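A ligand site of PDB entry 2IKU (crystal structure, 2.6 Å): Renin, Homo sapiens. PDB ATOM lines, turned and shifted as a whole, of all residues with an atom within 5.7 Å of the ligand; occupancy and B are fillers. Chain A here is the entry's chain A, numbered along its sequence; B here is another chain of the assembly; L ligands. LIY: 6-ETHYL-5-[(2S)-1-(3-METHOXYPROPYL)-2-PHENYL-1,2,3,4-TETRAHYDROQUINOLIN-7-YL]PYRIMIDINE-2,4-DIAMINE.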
ATOM      1  N   THR A  18      18.893  -2.471  19.497  1.00  0.00           N
ATOM      2  CA  THR A  18      17.735  -1.572  19.566  1.00  0.00           C
ATOM      3  C   THR A  18      17.362  -1.165  20.985  1.00  0.00           C
ATOM      4  O   THR A  18      16.598  -0.232  21.160  1.00  0.00           O
ATOM      5  CB  THR A  18      16.497  -2.194  18.907  1.00  0.00           C
ATOM      6  OG1 THR A  18      16.243  -3.476  19.500  1.00  0.00           O
ATOM      7  CG2 THR A  18      16.719  -2.361  17.418  1.00  0.00           C
ATOM      8  N   GLN A  19      17.910  -1.863  21.982  1.00  0.00           N
ATOM      9  CA  GLN A  19      17.674  -1.521  23.387  1.00  0.00           C
ATOM     10  C   GLN A  19      18.982  -1.675  24.168  1.00  0.00           C
ATOM     11  O   GLN A  19      19.623  -2.726  24.106  1.00  0.00           O
ATOM     12  CB  GLN A  19      16.589  -2.443  23.964  1.00  0.00           C
ATOM     13  CG  GLN A  19      15.274  -2.420  23.194  1.00  0.00           C
ATOM     14  CD  GLN A  19      14.221  -3.349  23.751  1.00  0.00           C
ATOM     15  OE1 GLN A  19      14.157  -3.602  24.965  1.00  0.00           O
ATOM     16  NE2 GLN A  19      13.363  -3.862  22.873  1.00  0.00           N
ATOM     17  N   TYR A  20      19.360  -0.613  24.862  1.00  0.00           N
ATOM     18  CA  TYR A  20      20.522  -0.571  25.745  1.00  0.00           C
ATOM     19  C   TYR A  20      20.043  -0.233  27.165  1.00  0.00           C
ATOM     20  O   TYR A  20      19.328   0.773  27.380  1.00  0.00           O
ATOM     21  CB  TYR A  20      21.495   0.492  25.253  1.00  0.00           C
ATOM     22  CG  TYR A  20      22.122   0.191  23.892  1.00  0.00           C
ATOM     23  CD1 TYR A  20      21.457   0.521  22.699  1.00  0.00           C
ATOM     24  CD2 TYR A  20      23.353  -0.441  23.793  1.00  0.00           C
ATOM     25  CE1 TYR A  20      22.031   0.250  21.471  1.00  0.00           C
ATOM     26  CE2 TYR A  20      23.933  -0.703  22.581  1.00  0.00           C
ATOM     27  CZ  TYR A  20      23.266  -0.354  21.426  1.00  0.00           C
ATOM     28  OH  TYR A  20      23.853  -0.631  20.231  1.00  0.00           O
ATOM     29  N   VAL A  36      16.468   1.731  30.830  1.00  0.00           N
ATOM     30  CA  VAL A  36      17.149   2.495  29.768  1.00  0.00           C
ATOM     31  C   VAL A  36      17.483   3.889  30.274  1.00  0.00           C
ATOM     32  O   VAL A  36      16.628   4.572  30.817  1.00  0.00           O
ATOM     33  CB  VAL A  36      16.268   2.646  28.528  1.00  0.00           C
ATOM     34  CG1 VAL A  36      16.933   3.561  27.502  1.00  0.00           C
ATOM     35  CG2 VAL A  36      15.940   1.290  27.943  1.00  0.00           C
ATOM     36  N   ASP A  38      17.861   7.478  29.482  1.00  0.00           N
ATOM     37  CA  ASP A  38      17.145   8.107  28.367  1.00  0.00           C
ATOM     38  C   ASP A  38      17.220   9.613  28.412  1.00  0.00           C
ATOM     39  O   ASP A  38      16.589  10.246  29.255  1.00  0.00           O
ATOM     40  CB  ASP A  38      15.694   7.633  28.408  1.00  0.00           C
ATOM     41  CG  ASP A  38      14.806   8.312  27.407  1.00  0.00           C
ATOM     42  OD1 ASP A  38      13.584   8.095  27.464  1.00  0.00           O
ATOM     43  OD2 ASP A  38      15.329   9.075  26.576  1.00  0.00           O
ATOM     44  N   THR A  39      17.967  10.202  27.475  1.00  0.00           N
ATOM     45  CA  THR A  39      18.098  11.666  27.382  1.00  0.00           C
ATOM     46  C   THR A  39      16.910  12.344  26.742  1.00  0.00           C
ATOM     47  O   THR A  39      16.810  13.561  26.782  1.00  0.00           O
ATOM     48  CB  THR A  39      19.336  12.062  26.587  1.00  0.00           C
ATOM     49  OG1 THR A  39      19.339  11.370  25.320  1.00  0.00           O
ATOM     50  CG2 THR A  39      20.626  11.764  27.411  1.00  0.00           C
ATOM     51  N   GLY A  40      16.013  11.564  26.153  1.00  0.00           N
ATOM     52  CA  GLY A  40      14.768  12.116  25.595  1.00  0.00           C
ATOM     53  C   GLY A  40      13.589  12.179  26.561  1.00  0.00           C
ATOM     54  O   GLY A  40      12.486  12.515  26.145  1.00  0.00           O
ATOM     55  N   SER A  41      13.782  11.811  27.816  1.00  0.00           N
ATOM     56  CA  SER A  41      12.752  12.015  28.836  1.00  0.00           C
ATOM     57  C   SER A  41      13.401  12.352  30.177  1.00  0.00           C
ATOM     58  O   SER A  41      14.611  12.255  30.342  1.00  0.00           O
ATOM     59  CB  SER A  41      11.830  10.806  28.939  1.00  0.00           C
ATOM     60  OG  SER A  41      12.538   9.626  29.294  1.00  0.00           O
ATOM     61  N   TYR A  83       5.538   8.620  25.344  1.00  0.00           N
ATOM     62  CA  TYR A  83       6.705   8.455  24.470  1.00  0.00           C
ATOM     63  C   TYR A  83       6.237   8.284  23.029  1.00  0.00           C
ATOM     64  O   TYR A  83       5.076   7.975  22.783  1.00  0.00           O
ATOM     65  CB  TYR A  83       7.551   7.247  24.909  1.00  0.00           C
ATOM     66  CG  TYR A  83       7.973   7.247  26.368  1.00  0.00           C
ATOM     67  CD1 TYR A  83       7.282   6.494  27.299  1.00  0.00           C
ATOM     68  CD2 TYR A  83       9.069   7.986  26.794  1.00  0.00           C
ATOM     69  CE1 TYR A  83       7.658   6.478  28.631  1.00  0.00           C
ATOM     70  CE2 TYR A  83       9.450   7.986  28.127  1.00  0.00           C
ATOM     71  CZ  TYR A  83       8.733   7.236  29.042  1.00  0.00           C
ATOM     72  OH  TYR A  83       9.100   7.224  30.363  1.00  0.00           O
ATOM     73  N   SER A  84       7.143   8.453  22.086  1.00  0.00           N
ATOM     74  CA  SER A  84       6.826   8.354  20.675  1.00  0.00           C
ATOM     75  C   SER A  84       6.272   6.991  20.252  1.00  0.00           C
ATOM     76  O   SER A  84       5.543   6.908  19.254  1.00  0.00           O
ATOM     77  CB  SER A  84       8.062   8.651  19.848  1.00  0.00           C
ATOM     78  OG  SER A  84       9.096   7.750  20.162  1.00  0.00           O
ATOM     79  N   THR A  85       6.621   5.941  21.002  1.00  0.00           N
ATOM     80  CA  THR A  85       6.198   4.582  20.661  1.00  0.00           C
ATOM     81  C   THR A  85       5.246   3.960  21.684  1.00  0.00           C
ATOM     82  O   THR A  85       4.884   2.791  21.554  1.00  0.00           O
ATOM     83  CB  THR A  85       7.427   3.675  20.549  1.00  0.00           C
ATOM     84  OG1 THR A  85       8.107   3.666  21.797  1.00  0.00           O
ATOM     85  CG2 THR A  85       8.365   4.186  19.481  1.00  0.00           C
ATOM     86  N   GLY A  86       4.839   4.728  22.688  1.00  0.00           N
ATOM     87  CA  GLY A  86       3.870   4.235  23.663  1.00  0.00           C
ATOM     88  C   GLY A  86       3.736   5.078  24.911  1.00  0.00           C
ATOM     89  O   GLY A  86       4.470   6.026  25.119  1.00  0.00           O
ATOM     90  N   PRO A 118       3.733  -1.417  23.237  1.00  0.00           N
ATOM     91  CA  PRO A 118       4.933  -2.167  22.916  1.00  0.00           C
ATOM     92  C   PRO A 118       5.673  -2.814  24.091  1.00  0.00           C
ATOM     93  O   PRO A 118       6.753  -3.359  23.882  1.00  0.00           O
ATOM     94  CB  PRO A 118       5.801  -1.091  22.335  1.00  0.00           C
ATOM     95  CG  PRO A 118       5.545   0.058  23.270  1.00  0.00           C
ATOM     96  CD  PRO A 118       4.084  -0.038  23.628  1.00  0.00           C
ATOM     97  N   PHE A 119       5.152  -2.749  25.312  1.00  0.00           N
ATOM     98  CA  PHE A 119       6.011  -3.074  26.436  1.00  0.00           C
ATOM     99  C   PHE A 119       6.359  -4.536  26.611  1.00  0.00           C
ATOM    100  O   PHE A 119       7.348  -4.834  27.280  1.00  0.00           O
ATOM    101  CB  PHE A 119       5.523  -2.430  27.716  1.00  0.00           C
ATOM    102  CG  PHE A 119       5.775  -0.990  27.724  1.00  0.00           C
ATOM    103  CD1 PHE A 119       4.794  -0.110  27.367  1.00  0.00           C
ATOM    104  CD2 PHE A 119       7.047  -0.514  27.988  1.00  0.00           C
ATOM    105  CE1 PHE A 119       5.053   1.249  27.331  1.00  0.00           C
ATOM    106  CE2 PHE A 119       7.302   0.827  27.950  1.00  0.00           C
ATOM    107  CZ  PHE A 119       6.303   1.711  27.610  1.00  0.00           C
ATOM    108  N   LEU A 121       7.491  -6.052  24.100  1.00  0.00           N
ATOM    109  CA  LEU A 121       8.710  -6.115  23.320  1.00  0.00           C
ATOM    110  C   LEU A 121       9.904  -5.479  24.068  1.00  0.00           C
ATOM    111  O   LEU A 121      11.020  -5.553  23.574  1.00  0.00           O
ATOM    112  CB  LEU A 121       8.510  -5.504  21.932  1.00  0.00           C
ATOM    113  CG  LEU A 121       7.404  -6.118  21.050  1.00  0.00           C
ATOM    114  CD1 LEU A 121       7.229  -5.267  19.825  1.00  0.00           C
ATOM    115  CD2 LEU A 121       7.674  -7.575  20.592  1.00  0.00           C
ATOM    116  N   ALA A 122       9.683  -4.900  25.244  1.00  0.00           N
ATOM    117  CA  ALA A 122      10.786  -4.368  26.064  1.00  0.00           C
ATOM    118  C   ALA A 122      11.566  -5.448  26.811  1.00  0.00           C
ATOM    119  O   ALA A 122      10.986  -6.227  27.601  1.00  0.00           O
ATOM    120  CB  ALA A 122      10.268  -3.358  27.041  1.00  0.00           C
ATOM    121  N   PHE A 124      13.886  -4.314  28.693  1.00  0.00           N
ATOM    122  CA  PHE A 124      14.013  -3.581  29.931  1.00  0.00           C
ATOM    123  C   PHE A 124      12.689  -3.520  30.713  1.00  0.00           C
ATOM    124  O   PHE A 124      11.616  -3.755  30.178  1.00  0.00           O
ATOM    125  CB  PHE A 124      14.544  -2.165  29.645  1.00  0.00           C
ATOM    126  CG  PHE A 124      13.674  -1.361  28.727  1.00  0.00           C
ATOM    127  CD1 PHE A 124      13.874  -1.415  27.352  1.00  0.00           C
ATOM    128  CD2 PHE A 124      12.682  -0.535  29.233  1.00  0.00           C
ATOM    129  CE1 PHE A 124      13.089  -0.675  26.485  1.00  0.00           C
ATOM    130  CE2 PHE A 124      11.878   0.232  28.382  1.00  0.00           C
ATOM    131  CZ  PHE A 124      12.081   0.166  27.000  1.00  0.00           C
ATOM    132  N   GLY A 126      12.120  -0.709  33.081  1.00  0.00           N
ATOM    133  CA  GLY A 126      11.774   0.714  33.265  1.00  0.00           C
ATOM    134  C   GLY A 126      12.673   1.710  32.574  1.00  0.00           C
ATOM    135  O   GLY A 126      13.444   1.356  31.695  1.00  0.00           O
ATOM    136  N   VAL A 127      12.562   2.965  32.962  1.00  0.00           N
ATOM    137  CA  VAL A 127      13.310   4.025  32.326  1.00  0.00           C
ATOM    138  C   VAL A 127      13.844   4.976  33.385  1.00  0.00           C
ATOM    139  O   VAL A 127      13.172   5.267  34.379  1.00  0.00           O
ATOM    140  CB  VAL A 127      12.424   4.835  31.328  1.00  0.00           C
ATOM    141  CG1 VAL A 127      13.221   6.042  30.718  1.00  0.00           C
ATOM    142  CG2 VAL A 127      11.874   3.904  30.241  1.00  0.00           C
ATOM    143  N   TYR A 162      27.698   3.277  23.215  1.00  0.00           N
ATOM    144  CA  TYR A 162      26.846   2.165  22.755  1.00  0.00           C
ATOM    145  C   TYR A 162      27.620   1.315  21.785  1.00  0.00           C
ATOM    146  O   TYR A 162      27.866   1.727  20.651  1.00  0.00           O
ATOM    147  CB  TYR A 162      25.568   2.644  22.058  1.00  0.00           C
ATOM    148  CG  TYR A 162      24.424   3.122  22.931  1.00  0.00           C
ATOM    149  CD1 TYR A 162      23.302   3.686  22.349  1.00  0.00           C
ATOM    150  CD2 TYR A 162      24.447   3.014  24.312  1.00  0.00           C
ATOM    151  CE1 TYR A 162      22.254   4.145  23.105  1.00  0.00           C
ATOM    152  CE2 TYR A 162      23.376   3.459  25.083  1.00  0.00           C
ATOM    153  CZ  TYR A 162      22.285   4.025  24.466  1.00  0.00           C
ATOM    154  OH  TYR A 162      21.210   4.495  25.191  1.00  0.00           O
ATOM    155  N   ASP A 226      19.085  11.531  21.462  1.00  0.00           N
ATOM    156  CA  ASP A 226      18.170  10.731  22.270  1.00  0.00           C
ATOM    157  C   ASP A 226      18.697   9.334  22.515  1.00  0.00           C
ATOM    158  O   ASP A 226      18.445   8.427  21.747  1.00  0.00           O
ATOM    159  CB  ASP A 226      16.816  10.645  21.545  1.00  0.00           C
ATOM    160  CG  ASP A 226      15.717  10.062  22.399  1.00  0.00           C
ATOM    161  OD1 ASP A 226      14.552  10.137  21.950  1.00  0.00           O
ATOM    162  OD2 ASP A 226      15.966   9.551  23.521  1.00  0.00           O
ATOM    163  N   THR A 227      19.383   9.157  23.635  1.00  0.00           N
ATOM    164  CA  THR A 227      19.905   7.855  24.022  1.00  0.00           C
ATOM    165  C   THR A 227      18.832   6.772  24.218  1.00  0.00           C
ATOM    166  O   THR A 227      19.168   5.571  24.289  1.00  0.00           O
ATOM    167  CB  THR A 227      20.655   7.945  25.348  1.00  0.00           C
ATOM    168  OG1 THR A 227      19.752   8.463  26.365  1.00  0.00           O
ATOM    169  CG2 THR A 227      21.862   8.828  25.171  1.00  0.00           C
ATOM    170  N   GLY A 228      17.575   7.194  24.327  1.00  0.00           N
ATOM    171  CA  GLY A 228      16.443   6.288  24.537  1.00  0.00           C
ATOM    172  C   GLY A 228      15.661   5.918  23.269  1.00  0.00           C
ATOM    173  O   GLY A 228      14.673   5.204  23.344  1.00  0.00           O
ATOM    174  N   ALA A 229      16.103   6.425  22.114  1.00  0.00           N
ATOM    175  CA  ALA A 229      15.527   6.039  20.818  1.00  0.00           C
ATOM    176  C   ALA A 229      16.430   5.010  20.129  1.00  0.00           C
ATOM    177  O   ALA A 229      17.658   5.143  20.125  1.00  0.00           O
ATOM    178  CB  ALA A 229      15.353   7.268  19.930  1.00  0.00           C
ATOM    179  N   SER A 230      15.840   3.980  19.550  1.00  0.00           N
ATOM    180  CA  SER A 230      16.617   2.976  18.833  1.00  0.00           C
ATOM    181  C   SER A 230      17.320   3.557  17.634  1.00  0.00           C
ATOM    182  O   SER A 230      18.479   3.279  17.427  1.00  0.00           O
ATOM    183  CB  SER A 230      15.758   1.823  18.384  1.00  0.00           C
ATOM    184  OG  SER A 230      15.406   1.043  19.505  1.00  0.00           O
ATOM    185  N   ALA A 317      20.445   5.465  18.946  1.00  0.00           N
ATOM    186  CA  ALA A 317      21.512   4.441  18.971  1.00  0.00           C
ATOM    187  C   ALA A 317      22.270   4.277  17.650  1.00  0.00           C
ATOM    188  O   ALA A 317      23.497   4.073  17.639  1.00  0.00           O
ATOM    189  CB  ALA A 317      20.940   3.093  19.401  1.00  0.00           C
ATOM    190  N   TYR B  60      -0.238   5.803  17.117  1.00  0.00           N
ATOM    191  CA  TYR B  60       0.285   5.537  15.751  1.00  0.00           C
ATOM    192  C   TYR B  60      -0.681   5.909  14.628  1.00  0.00           C
ATOM    193  O   TYR B  60      -0.483   5.496  13.470  1.00  0.00           O
ATOM    194  CB  TYR B  60       0.677   4.057  15.604  1.00  0.00           C
ATOM    195  CG  TYR B  60       2.011   3.691  16.225  1.00  0.00           C
ATOM    196  CD1 TYR B  60       2.161   3.525  17.603  1.00  0.00           C
ATOM    197  CD2 TYR B  60       3.122   3.485  15.412  1.00  0.00           C
ATOM    198  CE1 TYR B  60       3.377   3.185  18.169  1.00  0.00           C
ATOM    199  CE2 TYR B  60       4.358   3.154  15.956  1.00  0.00           C
ATOM    200  CZ  TYR B  60       4.489   2.999  17.335  1.00  0.00           C
ATOM    201  OH  TYR B  60       5.747   2.665  17.849  1.00  0.00           O
HETATM  202  N1  LIY L   1      11.706   7.447  23.290  1.00  0.00           N
HETATM  203  N3  LIY L   1      10.413   5.882  22.155  1.00  0.00           N
HETATM  204  C4  LIY L   1      11.078   5.447  24.489  1.00  0.00           C
HETATM  205  C6  LIY L   1      11.965   5.227  26.956  1.00  0.00           C
HETATM  206  C7  LIY L   1       9.283   3.742  25.093  1.00  0.00           C
HETATM  207  C8  LIY L   1       8.875   2.407  25.004  1.00  0.00           C
HETATM  208  C10 LIY L   1      10.897   1.845  23.711  1.00  0.00           C
HETATM  209  C13 LIY L   1       9.179   0.038  24.235  1.00  0.00           C
HETATM  210  C15 LIY L   1      11.204  -0.479  22.743  1.00  0.00           C
HETATM  211  C17 LIY L   1      14.042   1.417  23.538  1.00  0.00           C
HETATM  212  C20 LIY L   1      13.015   4.145  26.794  1.00  0.00           C
HETATM  213  C21 LIY L   1      10.440  -0.627  21.485  1.00  0.00           C
HETATM  214  C22 LIY L   1      10.309  -1.914  20.938  1.00  0.00           C
HETATM  215  C24 LIY L   1       9.011  -1.055  19.120  1.00  0.00           C
HETATM  216  C26 LIY L   1       9.829   0.452  20.832  1.00  0.00           C
HETATM  217  C1  LIY L   1      11.062   6.268  23.273  1.00  0.00           C
HETATM  218  C3  LIY L   1      11.831   5.975  25.653  1.00  0.00           C
HETATM  219  N2  LIY L   1      12.415   7.178  25.538  1.00  0.00           N
HETATM  220  C2  LIY L   1      12.375   7.878  24.379  1.00  0.00           C
HETATM  221  N4  LIY L   1      12.978   9.083  24.315  1.00  0.00           N
HETATM  222  C12 LIY L   1      10.464   4.103  24.487  1.00  0.00           C
HETATM  223  C11 LIY L   1      11.249   3.181  23.819  1.00  0.00           C
HETATM  224  C9  LIY L   1       9.631   1.451  24.340  1.00  0.00           C
HETATM  225  C14 LIY L   1      10.331  -0.903  23.909  1.00  0.00           C
HETATM  226  C23 LIY L   1       9.607  -2.123  19.761  1.00  0.00           C
HETATM  227  C25 LIY L   1       9.128   0.226  19.639  1.00  0.00           C
HETATM  228  N5  LIY L   1      11.668   0.894  23.016  1.00  0.00           N
HETATM  229  C16 LIY L   1      13.006   1.174  22.432  1.00  0.00           C
HETATM  230  C18 LIY L   1      15.313   2.016  22.944  1.00  0.00           C
HETATM  231  O1  LIY L   1      16.403   2.089  23.871  1.00  0.00           O
HETATM  232  C19 LIY L   1      17.574   2.719  23.296  1.00  0.00           C
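A nitrogen (N3) of the ligand is in hydrogen-bond range of the side-chain hydroxyl of Thr 85, at 3.2 Å.
The side-chain carboxylate (OD1) of Asp 38 is in hydrogen-bond range of a nitrogen (N2) of the ligand.
OD1 of Asp 226 lies within hydrogen-bond range of N4 of the ligand (3.0 Å).
The side-chain hydroxyl of Ser 84 sits at hydrogen-bond distance from a nitrogen (N3) of the ligand.
N of Gly 228 is in hydrogen-bond range of OD2 of Asp 226 (3.0 Å).
The backbone carbonyl oxygen (O) of Thr 227 sits at hydrogen-bond distance from the side-chain hydroxyl (OH) of Tyr 162, 2.5 Å away.
The side-chain hydroxyl (OG) of Ser 41 sits at hydrogen-bond distance from the side-chain carboxylate (OD1) of Asp 38 (2.6 Å).
The side-chain carboxylate (OD2) of Asp 226 is in hydrogen-bond range of the backbone NH (N) of Ala 229, 3.4 Å away.
The side-chain carboxylate (OD2) of Asp 226 is in hydrogen-bond range of the backbone NH (N) of Gly 40.
The backbone carbonyl oxygen of Gly 126 is in hydrogen-bond range of the backbone NH of Val 36, 3.2 Å away.
The backbone NH (N) of Thr 39 sits at hydrogen-bond distance from the side-chain hydroxyl (OG1) of Thr 227.
The backbone NH (N) of Ala 317 sits close to the backbone carbonyl oxygen (O) of Ser 230, at 3.3 Å.
Thr 18 touches the ligand (O to C18, 3.1 Å).
Gln 19 touches the ligand (CA to O1, 3.9 Å).
CG1 of Val 36 touches O1 of the ligand, 3.95 Å away.
Gly 40 touches the ligand (CA to N4, 3.7 Å).
CD2 of Tyr 83 touches C3 of the ligand, 3.6 Å away.
Pro 118 touches the ligand.
CE2 of Phe 119 touches C8 of the ligand, 3.7 Å away.
Leu 121 touches the ligand.
CB of Ala 122 touches C14 of the ligand (3.98 Å).
Phe 124 touches the ligand (CZ to C14, 3.7 Å).
Val 127 touches the ligand.
Thr 227 touches the ligand (O to C19, 3.4 Å).
Gly 228 touches the ligand (O to C18, 3.3 Å).
Ala 229 touches the ligand (O to C19, 3.99 Å).
OG of Ser 230 touches C18 of the ligand, at 3.6 Å.
Of the 27 residues printed, 19 come within 4 Å of the ligand.
The nearest printed residue that does not touch the ligand is Tyr 20 (4.1 Å).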
